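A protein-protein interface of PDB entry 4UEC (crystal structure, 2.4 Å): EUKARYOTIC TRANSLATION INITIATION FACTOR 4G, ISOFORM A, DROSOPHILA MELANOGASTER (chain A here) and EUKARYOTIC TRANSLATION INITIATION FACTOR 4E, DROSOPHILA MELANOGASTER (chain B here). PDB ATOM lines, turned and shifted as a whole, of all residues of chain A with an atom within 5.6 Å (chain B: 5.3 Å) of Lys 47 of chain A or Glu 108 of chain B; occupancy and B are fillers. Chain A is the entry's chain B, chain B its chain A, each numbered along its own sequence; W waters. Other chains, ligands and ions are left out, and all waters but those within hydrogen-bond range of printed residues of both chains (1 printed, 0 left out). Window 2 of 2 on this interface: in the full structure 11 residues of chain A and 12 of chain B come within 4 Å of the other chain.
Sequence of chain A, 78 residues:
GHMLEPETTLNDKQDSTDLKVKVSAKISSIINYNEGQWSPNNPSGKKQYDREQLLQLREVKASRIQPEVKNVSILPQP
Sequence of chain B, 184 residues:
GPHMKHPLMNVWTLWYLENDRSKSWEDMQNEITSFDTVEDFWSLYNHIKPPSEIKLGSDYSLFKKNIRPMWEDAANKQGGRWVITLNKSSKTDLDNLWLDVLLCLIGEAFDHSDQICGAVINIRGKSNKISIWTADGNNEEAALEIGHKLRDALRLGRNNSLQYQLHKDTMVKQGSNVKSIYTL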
ATOM      1  N   TRP A  38     -31.954  32.421  13.950  1.00  0.00           N
ATOM      2  CA  TRP A  38     -31.083  33.167  14.851  1.00  0.00           C
ATOM      3  C   TRP A  38     -30.352  34.288  14.118  1.00  0.00           C
ATOM      4  O   TRP A  38     -29.980  34.145  12.952  1.00  0.00           O
ATOM      5  CB  TRP A  38     -30.065  32.230  15.505  1.00  0.00           C
ATOM      6  CG  TRP A  38     -29.187  32.906  16.518  1.00  0.00           C
ATOM      7  CD1 TRP A  38     -29.345  32.900  17.874  1.00  0.00           C
ATOM      8  CD2 TRP A  38     -28.012  33.686  16.256  1.00  0.00           C
ATOM      9  NE1 TRP A  38     -28.344  33.627  18.472  1.00  0.00           N
ATOM     10  CE2 TRP A  38     -27.514  34.121  17.501  1.00  0.00           C
ATOM     11  CE3 TRP A  38     -27.334  34.060  15.091  1.00  0.00           C
ATOM     12  CZ2 TRP A  38     -26.370  34.910  17.613  1.00  0.00           C
ATOM     13  CZ3 TRP A  38     -26.199  34.844  15.204  1.00  0.00           C
ATOM     14  CH2 TRP A  38     -25.729  35.260  16.456  1.00  0.00           C
ATOM     15  N   GLY A  45     -33.941  33.489  17.966  1.00  0.00           N
ATOM     16  CA  GLY A  45     -34.232  32.642  16.822  1.00  0.00           C
ATOM     17  C   GLY A  45     -33.600  31.265  16.910  1.00  0.00           C
ATOM     18  O   GLY A  45     -32.710  31.028  17.727  1.00  0.00           O
ATOM     19  N   LYS A  46     -34.067  30.356  16.057  1.00  0.00           N
ATOM     20  CA  LYS A  46     -33.554  28.992  16.025  1.00  0.00           C
ATOM     21  C   LYS A  46     -32.214  28.934  15.300  1.00  0.00           C
ATOM     22  O   LYS A  46     -32.054  29.508  14.223  1.00  0.00           O
ATOM     23  CB  LYS A  46     -34.559  28.059  15.347  1.00  0.00           C
ATOM     24  CG  LYS A  46     -35.977  28.154  15.897  1.00  0.00           C
ATOM     25  CD  LYS A  46     -36.035  27.961  17.411  1.00  0.00           C
ATOM     26  CE  LYS A  46     -35.509  26.599  17.839  1.00  0.00           C
ATOM     27  NZ  LYS A  46     -35.576  26.420  19.314  1.00  0.00           N
ATOM     28  N   LYS A  47     -31.256  28.234  15.897  1.00  0.00           N
ATOM     29  CA  LYS A  47     -29.925  28.107  15.318  1.00  0.00           C
ATOM     30  C   LYS A  47     -29.923  27.067  14.198  1.00  0.00           C
ATOM     31  O   LYS A  47     -29.394  25.966  14.356  1.00  0.00           O
ATOM     32  CB  LYS A  47     -28.915  27.741  16.406  1.00  0.00           C
ATOM     33  CG  LYS A  47     -28.797  28.805  17.494  1.00  0.00           C
ATOM     34  CD  LYS A  47     -27.986  28.325  18.686  1.00  0.00           C
ATOM     35  CE  LYS A  47     -28.019  29.345  19.816  1.00  0.00           C
ATOM     36  NZ  LYS A  47     -27.437  28.817  21.082  1.00  0.00           N
ATOM     37  N   GLN A  48     -30.525  27.439  13.071  1.00  0.00           N
ATOM     38  CA  GLN A  48     -30.645  26.570  11.903  1.00  0.00           C
ATOM     39  C   GLN A  48     -30.180  27.327  10.661  1.00  0.00           C
ATOM     40  O   GLN A  48     -30.492  28.508  10.505  1.00  0.00           O
ATOM     41  CB  GLN A  48     -32.092  26.098  11.741  1.00  0.00           C
ATOM     42  CG  GLN A  48     -32.302  25.032  10.679  1.00  0.00           C
ATOM     43  CD  GLN A  48     -33.765  24.670  10.505  1.00  0.00           C
ATOM     44  OE1 GLN A  48     -34.656  25.445  10.857  1.00  0.00           O
ATOM     45  NE2 GLN A  48     -34.022  23.485   9.964  1.00  0.00           N
ATOM     46  N   TYR A  49     -29.440  26.652   9.781  1.00  0.00           N
ATOM     47  CA  TYR A  49     -28.846  27.312   8.617  1.00  0.00           C
ATOM     48  C   TYR A  49     -28.928  26.467   7.349  1.00  0.00           C
ATOM     49  O   TYR A  49     -28.654  25.267   7.370  1.00  0.00           O
ATOM     50  CB  TYR A  49     -27.380  27.654   8.898  1.00  0.00           C
ATOM     51  CG  TYR A  49     -27.157  28.448  10.166  1.00  0.00           C
ATOM     52  CD1 TYR A  49     -27.194  29.836  10.157  1.00  0.00           C
ATOM     53  CD2 TYR A  49     -26.903  27.806  11.372  1.00  0.00           C
ATOM     54  CE1 TYR A  49     -26.988  30.564  11.316  1.00  0.00           C
ATOM     55  CE2 TYR A  49     -26.695  28.526  12.533  1.00  0.00           C
ATOM     56  CZ  TYR A  49     -26.738  29.903  12.501  1.00  0.00           C
ATOM     57  OH  TYR A  49     -26.532  30.619  13.660  1.00  0.00           O
ATOM     58  N   PRO B   7     -23.737  31.167  16.165  1.00  0.00           N
ATOM     59  CA  PRO B   7     -23.659  29.936  16.960  1.00  0.00           C
ATOM     60  C   PRO B   7     -24.460  28.777  16.371  1.00  0.00           C
ATOM     61  O   PRO B   7     -25.523  28.985  15.786  1.00  0.00           O
ATOM     62  CB  PRO B   7     -24.242  30.361  18.308  1.00  0.00           C
ATOM     63  CG  PRO B   7     -25.232  31.405  17.956  1.00  0.00           C
ATOM     64  CD  PRO B   7     -24.657  32.146  16.774  1.00  0.00           C
ATOM     65  N   LEU B   8     -23.942  27.564  16.533  1.00  0.00           N
ATOM     66  CA  LEU B   8     -24.643  26.364  16.102  1.00  0.00           C
ATOM     67  C   LEU B   8     -25.584  25.885  17.202  1.00  0.00           C
ATOM     68  O   LEU B   8     -25.405  26.219  18.372  1.00  0.00           O
ATOM     69  CB  LEU B   8     -23.648  25.260  15.741  1.00  0.00           C
ATOM     70  CG  LEU B   8     -22.606  25.616  14.682  1.00  0.00           C
ATOM     71  CD1 LEU B   8     -21.562  24.515  14.578  1.00  0.00           C
ATOM     72  CD2 LEU B   8     -23.265  25.856  13.331  1.00  0.00           C
ATOM     73  N   MET B   9     -26.588  25.102  16.824  1.00  0.00           N
ATOM     74  CA  MET B   9     -27.533  24.562  17.792  1.00  0.00           C
ATOM     75  C   MET B   9     -26.842  23.579  18.736  1.00  0.00           C
ATOM     76  O   MET B   9     -27.257  23.415  19.883  1.00  0.00           O
ATOM     77  CB  MET B   9     -28.694  23.870  17.074  1.00  0.00           C
ATOM     78  CG  MET B   9     -29.840  23.464  17.987  1.00  0.00           C
ATOM     79  SD  MET B   9     -31.137  22.575  17.103  1.00  0.00           S
ATOM     80  CE  MET B   9     -31.815  23.877  16.074  1.00  0.00           C
ATOM     81  N   ASN B  10     -25.788  22.935  18.242  1.00  0.00           N
ATOM     82  CA  ASN B  10     -25.059  21.930  19.009  1.00  0.00           C
ATOM     83  C   ASN B  10     -23.548  22.109  18.927  1.00  0.00           C
ATOM     84  O   ASN B  10     -23.041  22.834  18.072  1.00  0.00           O
ATOM     85  CB  ASN B  10     -25.428  20.528  18.525  1.00  0.00           C
ATOM     86  CG  ASN B  10     -26.801  20.093  18.990  1.00  0.00           C
ATOM     87  OD1 ASN B  10     -26.973  19.656  20.128  1.00  0.00           O
ATOM     88  ND2 ASN B  10     -27.788  20.204  18.108  1.00  0.00           N
ATOM     89  N   TRP B  12     -20.082  20.225  18.146  1.00  0.00           N
ATOM     90  CA  TRP B  12     -19.638  19.069  17.373  1.00  0.00           C
ATOM     91  C   TRP B  12     -18.152  18.820  17.580  1.00  0.00           C
ATOM     92  O   TRP B  12     -17.396  19.748  17.865  1.00  0.00           O
ATOM     93  CB  TRP B  12     -19.935  19.277  15.888  1.00  0.00           C
ATOM     94  CG  TRP B  12     -21.387  19.516  15.593  1.00  0.00           C
ATOM     95  CD1 TRP B  12     -22.052  20.704  15.666  1.00  0.00           C
ATOM     96  CD2 TRP B  12     -22.353  18.541  15.176  1.00  0.00           C
ATOM     97  NE1 TRP B  12     -23.372  20.532  15.323  1.00  0.00           N
ATOM     98  CE2 TRP B  12     -23.582  19.213  15.018  1.00  0.00           C
ATOM     99  CE3 TRP B  12     -22.298  17.167  14.927  1.00  0.00           C
ATOM    100  CZ2 TRP B  12     -24.745  18.558  14.618  1.00  0.00           C
ATOM    101  CZ3 TRP B  12     -23.456  16.517  14.527  1.00  0.00           C
ATOM    102  CH2 TRP B  12     -24.662  17.213  14.380  1.00  0.00           C
ATOM    103  N   LYS B  64     -21.780  14.932  17.710  1.00  0.00           N
ATOM    104  CA  LYS B  64     -22.096  15.880  18.768  1.00  0.00           C
ATOM    105  C   LYS B  64     -21.188  15.628  19.966  1.00  0.00           C
ATOM    106  O   LYS B  64     -20.721  14.506  20.173  1.00  0.00           O
ATOM    107  CB  LYS B  64     -23.569  15.772  19.169  1.00  0.00           C
ATOM    108  CG  LYS B  64     -24.525  16.310  18.113  1.00  0.00           C
ATOM    109  CD  LYS B  64     -25.959  15.887  18.383  1.00  0.00           C
ATOM    110  CE  LYS B  64     -26.908  16.470  17.348  1.00  0.00           C
ATOM    111  NZ  LYS B  64     -28.290  15.948  17.499  1.00  0.00           N
ATOM    112  N   LEU B 103     -22.590  20.053   6.451  1.00  0.00           N
ATOM    113  CA  LEU B 103     -23.415  21.256   6.488  1.00  0.00           C
ATOM    114  C   LEU B 103     -24.848  20.937   6.913  1.00  0.00           C
ATOM    115  O   LEU B 103     -25.502  21.749   7.567  1.00  0.00           O
ATOM    116  CB  LEU B 103     -23.411  21.953   5.123  1.00  0.00           C
ATOM    117  CG  LEU B 103     -22.058  22.498   4.656  1.00  0.00           C
ATOM    118  CD1 LEU B 103     -22.160  23.045   3.238  1.00  0.00           C
ATOM    119  CD2 LEU B 103     -21.533  23.567   5.602  1.00  0.00           C
ATOM    120  N   CYS B 104     -25.333  19.757   6.544  1.00  0.00           N
ATOM    121  CA  CYS B 104     -26.651  19.314   6.984  1.00  0.00           C
ATOM    122  C   CYS B 104     -26.674  19.159   8.500  1.00  0.00           C
ATOM    123  O   CYS B 104     -27.636  19.546   9.164  1.00  0.00           O
ATOM    124  CB  CYS B 104     -27.034  17.991   6.319  1.00  0.00           C
ATOM    125  SG  CYS B 104     -27.679  18.150   4.643  1.00  0.00           S
ATOM    126  N   LEU B 105     -25.601  18.590   9.039  1.00  0.00           N
ATOM    127  CA  LEU B 105     -25.503  18.334  10.470  1.00  0.00           C
ATOM    128  C   LEU B 105     -25.424  19.629  11.271  1.00  0.00           C
ATOM    129  O   LEU B 105     -26.261  19.874  12.139  1.00  0.00           O
ATOM    130  CB  LEU B 105     -24.287  17.452  10.770  1.00  0.00           C
ATOM    131  CG  LEU B 105     -24.550  15.943  10.841  1.00  0.00           C
ATOM    132  CD1 LEU B 105     -25.372  15.456   9.659  1.00  0.00           C
ATOM    133  CD2 LEU B 105     -23.234  15.178  10.920  1.00  0.00           C
ATOM    134  N   ILE B 106     -24.426  20.461  10.980  1.00  0.00           N
ATOM    135  CA  ILE B 106     -24.210  21.675  11.765  1.00  0.00           C
ATOM    136  C   ILE B 106     -25.328  22.685  11.528  1.00  0.00           C
ATOM    137  O   ILE B 106     -25.594  23.539  12.375  1.00  0.00           O
ATOM    138  CB  ILE B 106     -22.842  22.329  11.452  1.00  0.00           C
ATOM    139  CG1 ILE B 106     -22.813  22.922  10.039  1.00  0.00           C
ATOM    140  CG2 ILE B 106     -21.720  21.312  11.645  1.00  0.00           C
ATOM    141  CD1 ILE B 106     -21.538  23.669   9.725  1.00  0.00           C
ATOM    142  N   GLY B 107     -25.983  22.578  10.377  1.00  0.00           N
ATOM    143  CA  GLY B 107     -27.096  23.448  10.044  1.00  0.00           C
ATOM    144  C   GLY B 107     -28.423  22.961  10.602  1.00  0.00           C
ATOM    145  O   GLY B 107     -29.420  23.679  10.537  1.00  0.00           O
ATOM    146  N   GLU B 108     -28.433  21.746  11.149  1.00  0.00           N
ATOM    147  CA  GLU B 108     -29.650  21.140  11.691  1.00  0.00           C
ATOM    148  C   GLU B 108     -30.726  21.029  10.614  1.00  0.00           C
ATOM    149  O   GLU B 108     -31.849  21.500  10.790  1.00  0.00           O
ATOM    150  CB  GLU B 108     -30.179  21.948  12.880  1.00  0.00           C
ATOM    151  CG  GLU B 108     -29.166  22.167  13.991  1.00  0.00           C
ATOM    152  CD  GLU B 108     -28.786  20.883  14.704  1.00  0.00           C
ATOM    153  OE1 GLU B 108     -29.469  19.857  14.498  1.00  0.00           O
ATOM    154  OE2 GLU B 108     -27.802  20.900  15.473  1.00  0.00           O
ATOM    155  N   ALA B 109     -30.371  20.402   9.499  1.00  0.00           N
ATOM    156  CA  ALA B 109     -31.275  20.286   8.361  1.00  0.00           C
ATOM    157  C   ALA B 109     -32.453  19.371   8.673  1.00  0.00           C
ATOM    158  O   ALA B 109     -33.542  19.540   8.126  1.00  0.00           O
ATOM    159  CB  ALA B 109     -30.522  19.771   7.146  1.00  0.00           C
ATOM    160  N   PHE B 110     -32.228  18.408   9.558  1.00  0.00           N
ATOM    161  CA  PHE B 110     -33.229  17.393   9.857  1.00  0.00           C
ATOM    162  C   PHE B 110     -34.191  17.851  10.946  1.00  0.00           C
ATOM    163  O   PHE B 110     -33.792  18.506  11.910  1.00  0.00           O
ATOM    164  CB  PHE B 110     -32.542  16.096  10.275  1.00  0.00           C
ATOM    165  CG  PHE B 110     -31.442  15.675   9.347  1.00  0.00           C
ATOM    166  CD1 PHE B 110     -31.734  15.115   8.114  1.00  0.00           C
ATOM    167  CD2 PHE B 110     -30.116  15.841   9.704  1.00  0.00           C
ATOM    168  CE1 PHE B 110     -30.724  14.728   7.257  1.00  0.00           C
ATOM    169  CE2 PHE B 110     -29.102  15.455   8.852  1.00  0.00           C
ATOM    170  CZ  PHE B 110     -29.405  14.898   7.627  1.00  0.00           C
ATOM    171  N   SER B 113     -33.623  16.692  14.955  1.00  0.00           N
ATOM    172  CA  SER B 113     -32.241  17.022  15.287  1.00  0.00           C
ATOM    173  C   SER B 113     -31.759  16.206  16.483  1.00  0.00           C
ATOM    174  O   SER B 113     -30.616  15.752  16.518  1.00  0.00           O
ATOM    175  CB  SER B 113     -32.100  18.516  15.578  1.00  0.00           C
ATOM    176  OG  SER B 113     -32.225  19.280  14.390  1.00  0.00           O
HETATM  177  O   HOH W   1     -26.895  25.194  14.103  1.00  0.00           O
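The backbone carbonyl oxygen of Pro 7 of chain B is in hydrogen-bond range of the side-chain hydroxyl of Tyr 49 of chain A (2.9 Å).
N of Tyr 49 of chain A lies within hydrogen-bond range of O of Gly 107 of chain B, 3.1 Å away.
O of Glu 108 of chain B sits at hydrogen-bond distance from NE2 of Gln 48 of chain A (3.1 Å).
O of Lys 46 of chain A lies within hydrogen-bond range of N of Trp 38 of chain A (2.9 Å).
The side-chain amide nitrogen (ND2) of Asn 10 of chain B sits at hydrogen-bond distance from the side-chain carboxylate (OE2) of Glu 108 of chain B (2.7 Å).
The side-chain carboxylate of Glu 108 of chain B sits at hydrogen-bond distance from the side-chain hydroxyl of Ser 113 of chain B (2.8 Å).
Pro 7 of chain B touches Trp 38 of chain A.
Lys 47 of chain A touches Pro 7 of chain B.
Lys 47 of chain A touches Leu 8 of chain B.
Met 9 of chain B touches Lys 47 of chain A.
O of Lys 47 of chain A touches CG of Glu 108 of chain B (3.8 Å).
Gln 48 of chain A touches Gly 107 of chain B (CG to O, 3.2 Å).
Printed residues of chain B within 4 Å of Lys 47 of chain A: Pro 7, Leu 8, Met 9 and Glu 108.
Of chain A, only Lys 47 (3.8 Å) and Gln 48 (3.1 Å) come within 4 Å of Glu 108 of chain B.
Of the printed residues of chain A, Pro 7 of chain B touches Trp 38 (3.3 Å), Lys 47 (3.7 Å) and Tyr 49 (2.9 Å).
Of the printed residues of chain B, Trp 38 of chain A touches Pro 7 (3.3 Å).
Of the printed residues of chain B, Gln 48 of chain A touches Gly 107 (3.2 Å) and Glu 108 (3.1 Å).
Trp 12 of chain B touches none of the printed residues of chain A.
Ser 113 of chain B touches none of the printed residues of chain A.
The nearest residue of chain B that does not touch Lys 47 of chain A is Gly 107 of chain B (4.5 Å).
Of the 15 printed residues of chain B, 5 touch a printed residue of chain A.
Hydrophobic or aromatic side chains of chain B within 4 Å of the printed part of chain A: Pro 7 and Met 9.
Of the 6 printed residues of chain A, 4 touch a printed residue of chain B.
Hydrophobic or aromatic side chains of chain A that line the printed part of chain B: Trp 38 and Tyr 49.
Among the printed residues, no Asp or Glu carboxylate lies within 4 Å of a Lys or Arg side-chain nitrogen of the other chain.
Water W1 lies within hydrogen-bond range of the backbone carbonyl oxygen (O) of Lys 47 of chain A, the backbone carbonyl oxygen (O) of Ile 106 of chain B and the backbone NH (N) of Met 9 of chain B.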
